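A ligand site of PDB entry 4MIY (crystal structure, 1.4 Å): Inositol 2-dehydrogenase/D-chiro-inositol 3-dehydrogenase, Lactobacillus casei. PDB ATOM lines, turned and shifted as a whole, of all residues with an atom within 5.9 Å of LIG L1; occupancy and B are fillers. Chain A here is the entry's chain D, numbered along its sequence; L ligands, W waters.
Water W3 lies within hydrogen-bond range of an oxygen (O3) of LIG L1, the side-chain hydroxyl of Tyr 236 and the guanidinium group of Arg 127.
Water W2 lies within hydrogen-bond range of an oxygen (O8) of LG2 L2 (2.8 Å) and an oxygen (O1) of LIG L1 (2.9 Å).
O3 of LIG L1 is in hydrogen-bond range of O14 of LG2 L2, 2.9 Å away.
O of Lys 97 is in hydrogen-bond range of O12 of LG2 L2.
A ring nitrogen (NE2) of His 155 is in hydrogen-bond range of an oxygen (O4) of LIG L1 (2.6 Å).
The side-chain hydroxyl of Tyr 282 is in hydrogen-bond range of an oxygen (O14) of LG2 L2 (2.6 Å).
An oxygen (O5) of LIG L1 is in hydrogen-bond range of the side-chain amide oxygen of Asn 157, at 2.7 Å.
An oxygen (O6) of LIG L1 is in hydrogen-bond range of the side-chain carboxylate (OD2) of Asp 172, at 2.9 Å.
An oxygen (O2) of LIG L1 is in hydrogen-bond range of a ring nitrogen (NE2) of His 176, 2.7 Å away.
The side-chain amino group of Lys 97 lies within hydrogen-bond range of an oxygen (O13) of LG2 L2, at 2.9 Å.
O2 of LIG L1 sits at hydrogen-bond distance from NZ of Lys 97 (2.4 Å).
The side-chain hydroxyl (OH) of Tyr 236 sits at hydrogen-bond distance from an oxygen (O4) of LIG L1, 2.8 Å away.
The side-chain carboxylate (OD1) of Asp 172 sits at hydrogen-bond distance from an oxygen (O13) of LG2 L2, at 3.0 Å.
SD of Met 126 lies within hydrogen-bond range of N7 of LG2 L2, at 3.7 Å.
An oxygen (O2) of LIG L1 sits at hydrogen-bond distance from the backbone carbonyl oxygen of Asp 172, at 3.2 Å.
The side-chain hydroxyl (OG1) of Thr 173 sits at hydrogen-bond distance from an oxygen (O5) of LIG L1 (2.8 Å).
A ring nitrogen (ND1) of His 155 sits close to the guanidinium group of Arg 127 (3.4 Å).
A ring nitrogen (ND1) of His 155 lies close to the backbone carbonyl oxygen (O) of Thr 173 (3.3 Å).
The side-chain hydroxyl (OG1) of Thr 173 lies within hydrogen-bond range of the side-chain hydroxyl (OH) of Tyr 164 (2.6 Å).
The side-chain carboxylate of Asp 172 is in salt-bridge range of the side-chain amino group of Lys 97 (3.9 Å).
CE2 of Tyr 164 touches O6 of LIG L1, 3.9 Å away.
Hydrophobic or aromatic side chains that line LIG L1: His 155, Tyr 164, His 176 and Tyr 236.
Eight residues have an atom within 4 Å of LIG L1: Lys 97, His 155, Asn 157, Tyr 164, Asp 172, Thr 173, His 176 and Tyr 236.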
ATOM      1  N   LYS A  97     -12.676  16.704  10.679  1.00  0.00           N
ATOM      2  CA  LYS A  97     -11.845  16.304  11.777  1.00  0.00           C
ATOM      3  C   LYS A  97     -10.580  15.573  11.296  1.00  0.00           C
ATOM      4  O   LYS A  97     -10.548  15.067  10.228  1.00  0.00           O
ATOM      5  CB  LYS A  97     -12.611  15.462  12.799  1.00  0.00           C
ATOM      6  CG  LYS A  97     -13.604  14.470  12.259  1.00  0.00           C
ATOM      7  CD  LYS A  97     -13.052  13.387  11.389  1.00  0.00           C
ATOM      8  CE  LYS A  97     -11.983  12.597  12.037  1.00  0.00           C
ATOM      9  NZ  LYS A  97     -11.509  11.518  11.124  1.00  0.00           N
ATOM     10  N   MET A 126     -19.444  14.855  13.048  1.00  0.00           N
ATOM     11  CA  MET A 126     -20.789  14.565  12.574  1.00  0.00           C
ATOM     12  C   MET A 126     -21.619  13.695  13.486  1.00  0.00           C
ATOM     13  O   MET A 126     -22.792  13.649  13.322  1.00  0.00           O
ATOM     14  CB  MET A 126     -20.760  13.946  11.167  1.00  0.00           C
ATOM     15  CG  MET A 126     -20.534  12.460  11.129  1.00  0.00           C
ATOM     16  SD  MET A 126     -18.904  11.989  11.675  1.00  0.00           S
ATOM     17  CE  MET A 126     -19.027  10.191  11.546  1.00  0.00           C
ATOM     18  N   ARG A 127     -20.964  12.997  14.415  1.00  0.00           N
ATOM     19  CA  ARG A 127     -21.673  12.084  15.297  1.00  0.00           C
ATOM     20  C   ARG A 127     -22.833  12.788  16.006  1.00  0.00           C
ATOM     21  O   ARG A 127     -23.832  12.212  16.223  1.00  0.00           O
ATOM     22  CB  ARG A 127     -20.735  11.463  16.344  1.00  0.00           C
ATOM     23  CG  ARG A 127     -19.605  10.566  15.855  1.00  0.00           C
ATOM     24  CD  ARG A 127     -20.072   9.198  15.450  1.00  0.00           C
ATOM     25  NE  ARG A 127     -18.969   8.354  15.092  1.00  0.00           N
ATOM     26  CZ  ARG A 127     -18.300   7.637  15.957  1.00  0.00           C
ATOM     27  NH1 ARG A 127     -18.662   7.639  17.214  1.00  0.00           N
ATOM     28  NH2 ARG A 127     -17.301   6.885  15.560  1.00  0.00           N
ATOM     29  N   HIS A 155     -15.667   1.398  17.978  1.00  0.00           N
ATOM     30  CA  HIS A 155     -15.400   2.062  16.728  1.00  0.00           C
ATOM     31  C   HIS A 155     -14.602   1.079  15.864  1.00  0.00           C
ATOM     32  O   HIS A 155     -13.446   0.872  16.042  1.00  0.00           O
ATOM     33  CB  HIS A 155     -14.636   3.345  16.986  1.00  0.00           C
ATOM     34  CG  HIS A 155     -14.562   4.251  15.822  1.00  0.00           C
ATOM     35  ND1 HIS A 155     -14.231   5.578  15.952  1.00  0.00           N
ATOM     36  CD2 HIS A 155     -14.769   4.040  14.507  1.00  0.00           C
ATOM     37  CE1 HIS A 155     -14.251   6.145  14.766  1.00  0.00           C
ATOM     38  NE2 HIS A 155     -14.563   5.226  13.870  1.00  0.00           N
ATOM     39  N   ILE A 156     -15.329   0.493  14.938  1.00  0.00           N
ATOM     40  CA  ILE A 156     -14.858  -0.625  14.170  1.00  0.00           C
ATOM     41  C   ILE A 156     -14.692  -0.209  12.701  1.00  0.00           C
ATOM     42  O   ILE A 156     -15.565   0.343  12.145  1.00  0.00           O
ATOM     43  CB  ILE A 156     -15.859  -1.775  14.230  1.00  0.00           C
ATOM     44  CG1 ILE A 156     -16.196  -2.173  15.661  1.00  0.00           C
ATOM     45  CG2 ILE A 156     -15.339  -2.960  13.465  1.00  0.00           C
ATOM     46  CD1 ILE A 156     -15.054  -2.495  16.498  1.00  0.00           C
ATOM     47  N   ASN A 157     -13.531  -0.526  12.130  1.00  0.00           N
ATOM     48  CA  ASN A 157     -13.267  -0.322  10.716  1.00  0.00           C
ATOM     49  C   ASN A 157     -12.756  -1.644  10.156  1.00  0.00           C
ATOM     50  O   ASN A 157     -12.117  -2.339  10.836  1.00  0.00           O
ATOM     51  CB  ASN A 157     -12.152   0.686  10.448  1.00  0.00           C
ATOM     52  CG  ASN A 157     -12.466   2.120  10.864  1.00  0.00           C
ATOM     53  OD1 ASN A 157     -11.598   2.939  10.727  1.00  0.00           O
ATOM     54  ND2 ASN A 157     -13.638   2.409  11.324  1.00  0.00           N
ATOM     55  N   TYR A 164      -2.014   5.041   7.315  1.00  0.00           N
ATOM     56  CA  TYR A 164      -2.615   5.107   8.632  1.00  0.00           C
ATOM     57  C   TYR A 164      -1.594   4.729   9.703  1.00  0.00           C
ATOM     58  O   TYR A 164      -1.048   3.675   9.690  1.00  0.00           O
ATOM     59  CB  TYR A 164      -3.854   4.206   8.701  1.00  0.00           C
ATOM     60  CG  TYR A 164      -4.760   4.369   9.908  1.00  0.00           C
ATOM     61  CD1 TYR A 164      -4.438   3.809  11.118  1.00  0.00           C
ATOM     62  CD2 TYR A 164      -5.947   5.049   9.825  1.00  0.00           C
ATOM     63  CE1 TYR A 164      -5.261   3.939  12.180  1.00  0.00           C
ATOM     64  CE2 TYR A 164      -6.793   5.187  10.912  1.00  0.00           C
ATOM     65  CZ  TYR A 164      -6.442   4.609  12.077  1.00  0.00           C
ATOM     66  OH  TYR A 164      -7.245   4.683  13.155  1.00  0.00           O
ATOM     67  N   ASP A 172      -7.520  10.303  14.056  1.00  0.00           N
ATOM     68  CA  ASP A 172      -8.442  10.070  12.968  1.00  0.00           C
ATOM     69  C   ASP A 172      -9.663   9.316  13.435  1.00  0.00           C
ATOM     70  O   ASP A 172     -10.708   9.501  12.905  1.00  0.00           O
ATOM     71  CB  ASP A 172      -7.732   9.267  11.875  1.00  0.00           C
ATOM     72  CG  ASP A 172      -7.910   9.838  10.488  1.00  0.00           C
ATOM     73  OD1 ASP A 172      -7.712  11.028  10.294  1.00  0.00           O
ATOM     74  OD2 ASP A 172      -8.275   9.051   9.623  1.00  0.00           O
ATOM     75  N   THR A 173      -9.500   8.476  14.437  1.00  0.00           N
ATOM     76  CA  THR A 173     -10.536   7.509  14.767  1.00  0.00           C
ATOM     77  C   THR A 173     -11.196   7.815  16.123  1.00  0.00           C
ATOM     78  O   THR A 173     -12.306   8.201  16.172  1.00  0.00           O
ATOM     79  CB  THR A 173      -9.983   6.090  14.614  1.00  0.00           C
ATOM     80  OG1 THR A 173      -9.534   5.923  13.290  1.00  0.00           O
ATOM     81  CG2 THR A 173     -11.006   5.063  14.869  1.00  0.00           C
ATOM     82  N   ILE A 175     -10.905  10.238  17.949  1.00  0.00           N
ATOM     83  CA  ILE A 175     -11.327  11.617  18.009  1.00  0.00           C
ATOM     84  C   ILE A 175     -12.843  11.791  17.982  1.00  0.00           C
ATOM     85  O   ILE A 175     -13.358  12.634  18.604  1.00  0.00           O
ATOM     86  CB  ILE A 175     -10.611  12.487  16.935  1.00  0.00           C
ATOM     87  CG1 ILE A 175     -10.627  13.954  17.337  1.00  0.00           C
ATOM     88  CG2 ILE A 175     -11.228  12.368  15.614  1.00  0.00           C
ATOM     89  CD1 ILE A 175      -9.548  14.335  18.258  1.00  0.00           C
ATOM     90  N   HIS A 176     -13.525  10.929  17.258  1.00  0.00           N
ATOM     91  CA  HIS A 176     -14.964  10.970  17.207  1.00  0.00           C
ATOM     92  C   HIS A 176     -15.607  10.702  18.569  1.00  0.00           C
ATOM     93  O   HIS A 176     -16.480  11.418  18.991  1.00  0.00           O
ATOM     94  CB  HIS A 176     -15.492   9.928  16.227  1.00  0.00           C
ATOM     95  CG  HIS A 176     -15.315  10.316  14.785  1.00  0.00           C
ATOM     96  ND1 HIS A 176     -16.079  11.276  14.181  1.00  0.00           N
ATOM     97  CD2 HIS A 176     -14.480   9.859  13.845  1.00  0.00           C
ATOM     98  CE1 HIS A 176     -15.728  11.386  12.921  1.00  0.00           C
ATOM     99  NE2 HIS A 176     -14.752  10.543  12.691  1.00  0.00           N
ATOM    100  N   VAL A 230      -9.475  -1.177  14.021  1.00  0.00           N
ATOM    101  CA  VAL A 230      -9.469  -0.681  12.667  1.00  0.00           C
ATOM    102  C   VAL A 230      -9.024  -1.689  11.576  1.00  0.00           C
ATOM    103  O   VAL A 230      -9.041  -1.340  10.413  1.00  0.00           O
ATOM    104  CB  VAL A 230      -8.691   0.633  12.543  1.00  0.00           C
ATOM    105  CG1 VAL A 230      -9.294   1.651  13.467  1.00  0.00           C
ATOM    106  CG2 VAL A 230      -7.247   0.445  12.837  1.00  0.00           C
ATOM    107  N   TYR A 236     -17.742  -2.108   9.027  1.00  0.00           N
ATOM    108  CA  TYR A 236     -17.623  -0.805   9.647  1.00  0.00           C
ATOM    109  C   TYR A 236     -18.774  -0.660  10.607  1.00  0.00           C
ATOM    110  O   TYR A 236     -19.889  -0.831  10.227  1.00  0.00           O
ATOM    111  CB  TYR A 236     -17.708   0.297   8.599  1.00  0.00           C
ATOM    112  CG  TYR A 236     -17.585   1.662   9.180  1.00  0.00           C
ATOM    113  CD1 TYR A 236     -18.672   2.329   9.677  1.00  0.00           C
ATOM    114  CD2 TYR A 236     -16.362   2.276   9.252  1.00  0.00           C
ATOM    115  CE1 TYR A 236     -18.555   3.540  10.233  1.00  0.00           C
ATOM    116  CE2 TYR A 236     -16.244   3.494   9.780  1.00  0.00           C
ATOM    117  CZ  TYR A 236     -17.326   4.131  10.282  1.00  0.00           C
ATOM    118  OH  TYR A 236     -17.183   5.366  10.828  1.00  0.00           O
ATOM    119  N   TRP A 274     -17.819   4.310   6.425  1.00  0.00           N
ATOM    120  CA  TRP A 274     -18.442   5.500   6.963  1.00  0.00           C
ATOM    121  C   TRP A 274     -19.338   6.194   5.968  1.00  0.00           C
ATOM    122  O   TRP A 274     -20.274   6.830   6.336  1.00  0.00           O
ATOM    123  CB  TRP A 274     -17.352   6.472   7.441  1.00  0.00           C
ATOM    124  CG  TRP A 274     -16.214   6.562   6.534  1.00  0.00           C
ATOM    125  CD1 TRP A 274     -15.105   5.838   6.593  1.00  0.00           C
ATOM    126  CD2 TRP A 274     -16.089   7.405   5.382  1.00  0.00           C
ATOM    127  NE1 TRP A 274     -14.279   6.154   5.561  1.00  0.00           N
ATOM    128  CE2 TRP A 274     -14.874   7.102   4.788  1.00  0.00           C
ATOM    129  CE3 TRP A 274     -16.875   8.378   4.813  1.00  0.00           C
ATOM    130  CZ2 TRP A 274     -14.411   7.762   3.657  1.00  0.00           C
ATOM    131  CZ3 TRP A 274     -16.441   9.009   3.683  1.00  0.00           C
ATOM    132  CH2 TRP A 274     -15.226   8.698   3.118  1.00  0.00           C
ATOM    133  N   PHE A 278     -22.909   7.059   7.782  1.00  0.00           N
ATOM    134  CA  PHE A 278     -23.137   8.381   8.339  1.00  0.00           C
ATOM    135  C   PHE A 278     -23.586   9.431   7.322  1.00  0.00           C
ATOM    136  O   PHE A 278     -23.483  10.578   7.549  1.00  0.00           O
ATOM    137  CB  PHE A 278     -21.927   8.855   9.133  1.00  0.00           C
ATOM    138  CG  PHE A 278     -21.755   8.167  10.436  1.00  0.00           C
ATOM    139  CD1 PHE A 278     -22.653   8.337  11.434  1.00  0.00           C
ATOM    140  CD2 PHE A 278     -20.728   7.310  10.632  1.00  0.00           C
ATOM    141  CE1 PHE A 278     -22.506   7.700  12.604  1.00  0.00           C
ATOM    142  CE2 PHE A 278     -20.578   6.678  11.811  1.00  0.00           C
ATOM    143  CZ  PHE A 278     -21.483   6.874  12.795  1.00  0.00           C
ATOM    144  N   TYR A 282     -23.677  13.531   7.772  1.00  0.00           N
ATOM    145  CA  TYR A 282     -22.882  14.414   6.922  1.00  0.00           C
ATOM    146  C   TYR A 282     -23.772  15.397   6.158  1.00  0.00           C
ATOM    147  O   TYR A 282     -23.471  16.538   6.109  1.00  0.00           O
ATOM    148  CB  TYR A 282     -22.024  13.642   5.903  1.00  0.00           C
ATOM    149  CG  TYR A 282     -21.048  12.627   6.435  1.00  0.00           C
ATOM    150  CD1 TYR A 282     -20.157  12.929   7.406  1.00  0.00           C
ATOM    151  CD2 TYR A 282     -21.035  11.354   5.941  1.00  0.00           C
ATOM    152  CE1 TYR A 282     -19.284  11.979   7.891  1.00  0.00           C
ATOM    153  CE2 TYR A 282     -20.192  10.432   6.406  1.00  0.00           C
ATOM    154  CZ  TYR A 282     -19.328  10.710   7.386  1.00  0.00           C
ATOM    155  OH  TYR A 282     -18.488   9.728   7.827  1.00  0.00           O
HETATM  156  C1  LIG L   1     -12.072   8.252   9.111  1.00  0.00           C
HETATM  157  C2  LIG L   1     -13.332   8.807   9.697  1.00  0.00           C
HETATM  158  C3  LIG L   1     -14.263   7.691  10.090  1.00  0.00           C
HETATM  159  C4  LIG L   1     -13.604   6.808  11.082  1.00  0.00           C
HETATM  160  C5  LIG L   1     -12.348   6.218  10.542  1.00  0.00           C
HETATM  161  C6  LIG L   1     -11.384   7.374  10.165  1.00  0.00           C
HETATM  162  O1  LIG L   1     -11.230   9.321   8.759  1.00  0.00           O
HETATM  163  O2  LIG L   1     -13.058   9.680  10.763  1.00  0.00           O
HETATM  164  O3  LIG L   1     -15.488   8.283  10.597  1.00  0.00           O
HETATM  165  O4  LIG L   1     -14.500   5.753  11.333  1.00  0.00           O
HETATM  166  O5  LIG L   1     -11.726   5.476  11.554  1.00  0.00           O
HETATM  167  O6  LIG L   1     -10.142   6.842   9.629  1.00  0.00           O
HETATM  168  P1  LG2 L   2      -8.144  10.173   1.249  1.00  0.00           P
HETATM  169  O1  LG2 L   2      -6.803   9.675   1.470  1.00  0.00           O
HETATM  170  O2  LG2 L   2      -9.067   9.398   0.453  1.00  0.00           O
HETATM  171  O3  LG2 L   2      -8.048  11.619   0.628  1.00  0.00           O
HETATM  172  C1  LG2 L   2      -7.296  12.646   1.151  1.00  0.00           C
HETATM  173  C2  LG2 L   2      -6.943  13.541  -0.033  1.00  0.00           C
HETATM  174  O4  LG2 L   2      -6.217  14.636   0.456  1.00  0.00           O
HETATM  175  C3  LG2 L   2      -6.040  12.904  -1.038  1.00  0.00           C
HETATM  176  O5  LG2 L   2      -6.583  13.067  -2.321  1.00  0.00           O
HETATM  177  C4  LG2 L   2      -4.731  13.639  -0.930  1.00  0.00           C
HETATM  178  O6  LG2 L   2      -3.997  13.694  -2.127  1.00  0.00           O
HETATM  179  C5  LG2 L   2      -5.197  14.993  -0.485  1.00  0.00           C
HETATM  180  N1  LG2 L   2      -4.219  15.827   0.202  1.00  0.00           N
HETATM  181  C6  LG2 L   2      -3.307  15.468   1.099  1.00  0.00           C
HETATM  182  N2  LG2 L   2      -2.663  16.522   1.550  1.00  0.00           N
HETATM  183  C7  LG2 L   2      -3.148  17.582   0.956  1.00  0.00           C
HETATM  184  C8  LG2 L   2      -2.922  19.011   0.980  1.00  0.00           C
HETATM  185  N3  LG2 L   2      -1.968  19.491   1.732  1.00  0.00           N
HETATM  186  N4  LG2 L   2      -3.673  19.715   0.217  1.00  0.00           N
HETATM  187  C9  LG2 L   2      -4.570  19.191  -0.535  1.00  0.00           C
HETATM  188  N5  LG2 L   2      -4.864  17.941  -0.626  1.00  0.00           N
HETATM  189  C10 LG2 L   2      -4.170  17.104   0.090  1.00  0.00           C
HETATM  190  O7  LG2 L   2      -8.731  10.426   2.690  1.00  0.00           O
HETATM  191  P2  LG2 L   2     -10.192  10.792   3.191  1.00  0.00           P
HETATM  192  O8  LG2 L   2     -10.791   9.549   3.668  1.00  0.00           O
HETATM  193  O9  LG2 L   2     -10.900  11.552   2.143  1.00  0.00           O
HETATM  194  O10 LG2 L   2      -9.924  11.708   4.448  1.00  0.00           O
HETATM  195  C11 LG2 L   2      -9.793  13.085   4.290  1.00  0.00           C
HETATM  196  C12 LG2 L   2     -10.106  13.808   5.589  1.00  0.00           C
HETATM  197  O11 LG2 L   2     -11.469  13.559   5.873  1.00  0.00           O
HETATM  198  C13 LG2 L   2      -9.333  13.357   6.793  1.00  0.00           C
HETATM  199  O12 LG2 L   2      -9.197  14.478   7.650  1.00  0.00           O
HETATM  200  C14 LG2 L   2     -10.272  12.361   7.391  1.00  0.00           C
HETATM  201  O13 LG2 L   2      -9.987  12.226   8.762  1.00  0.00           O
HETATM  202  C15 LG2 L   2     -11.618  13.002   7.158  1.00  0.00           C
HETATM  203  N6  LG2 L   2     -12.733  12.070   7.178  1.00  0.00           N
HETATM  204  C16 LG2 L   2     -13.746  12.226   8.010  1.00  0.00           C
HETATM  205  C17 LG2 L   2     -14.826  11.360   8.028  1.00  0.00           C
HETATM  206  C18 LG2 L   2     -15.885  11.560   9.026  1.00  0.00           C
HETATM  207  O14 LG2 L   2     -16.516  10.612   9.310  1.00  0.00           O
HETATM  208  N7  LG2 L   2     -16.047  12.751   9.525  1.00  0.00           N
HETATM  209  C19 LG2 L   2     -14.854  10.280   7.154  1.00  0.00           C
HETATM  210  C20 LG2 L   2     -13.797  10.139   6.264  1.00  0.00           C
HETATM  211  C21 LG2 L   2     -12.745  11.054   6.308  1.00  0.00           C
HETATM  212  O   HOH W   1      -9.754   5.095   7.598  1.00  0.00           O
HETATM  213  O   HOH W   2     -10.127   8.534   6.211  1.00  0.00           O
HETATM  214  O   HOH W   3     -17.199   7.481  12.635  1.00  0.00           O
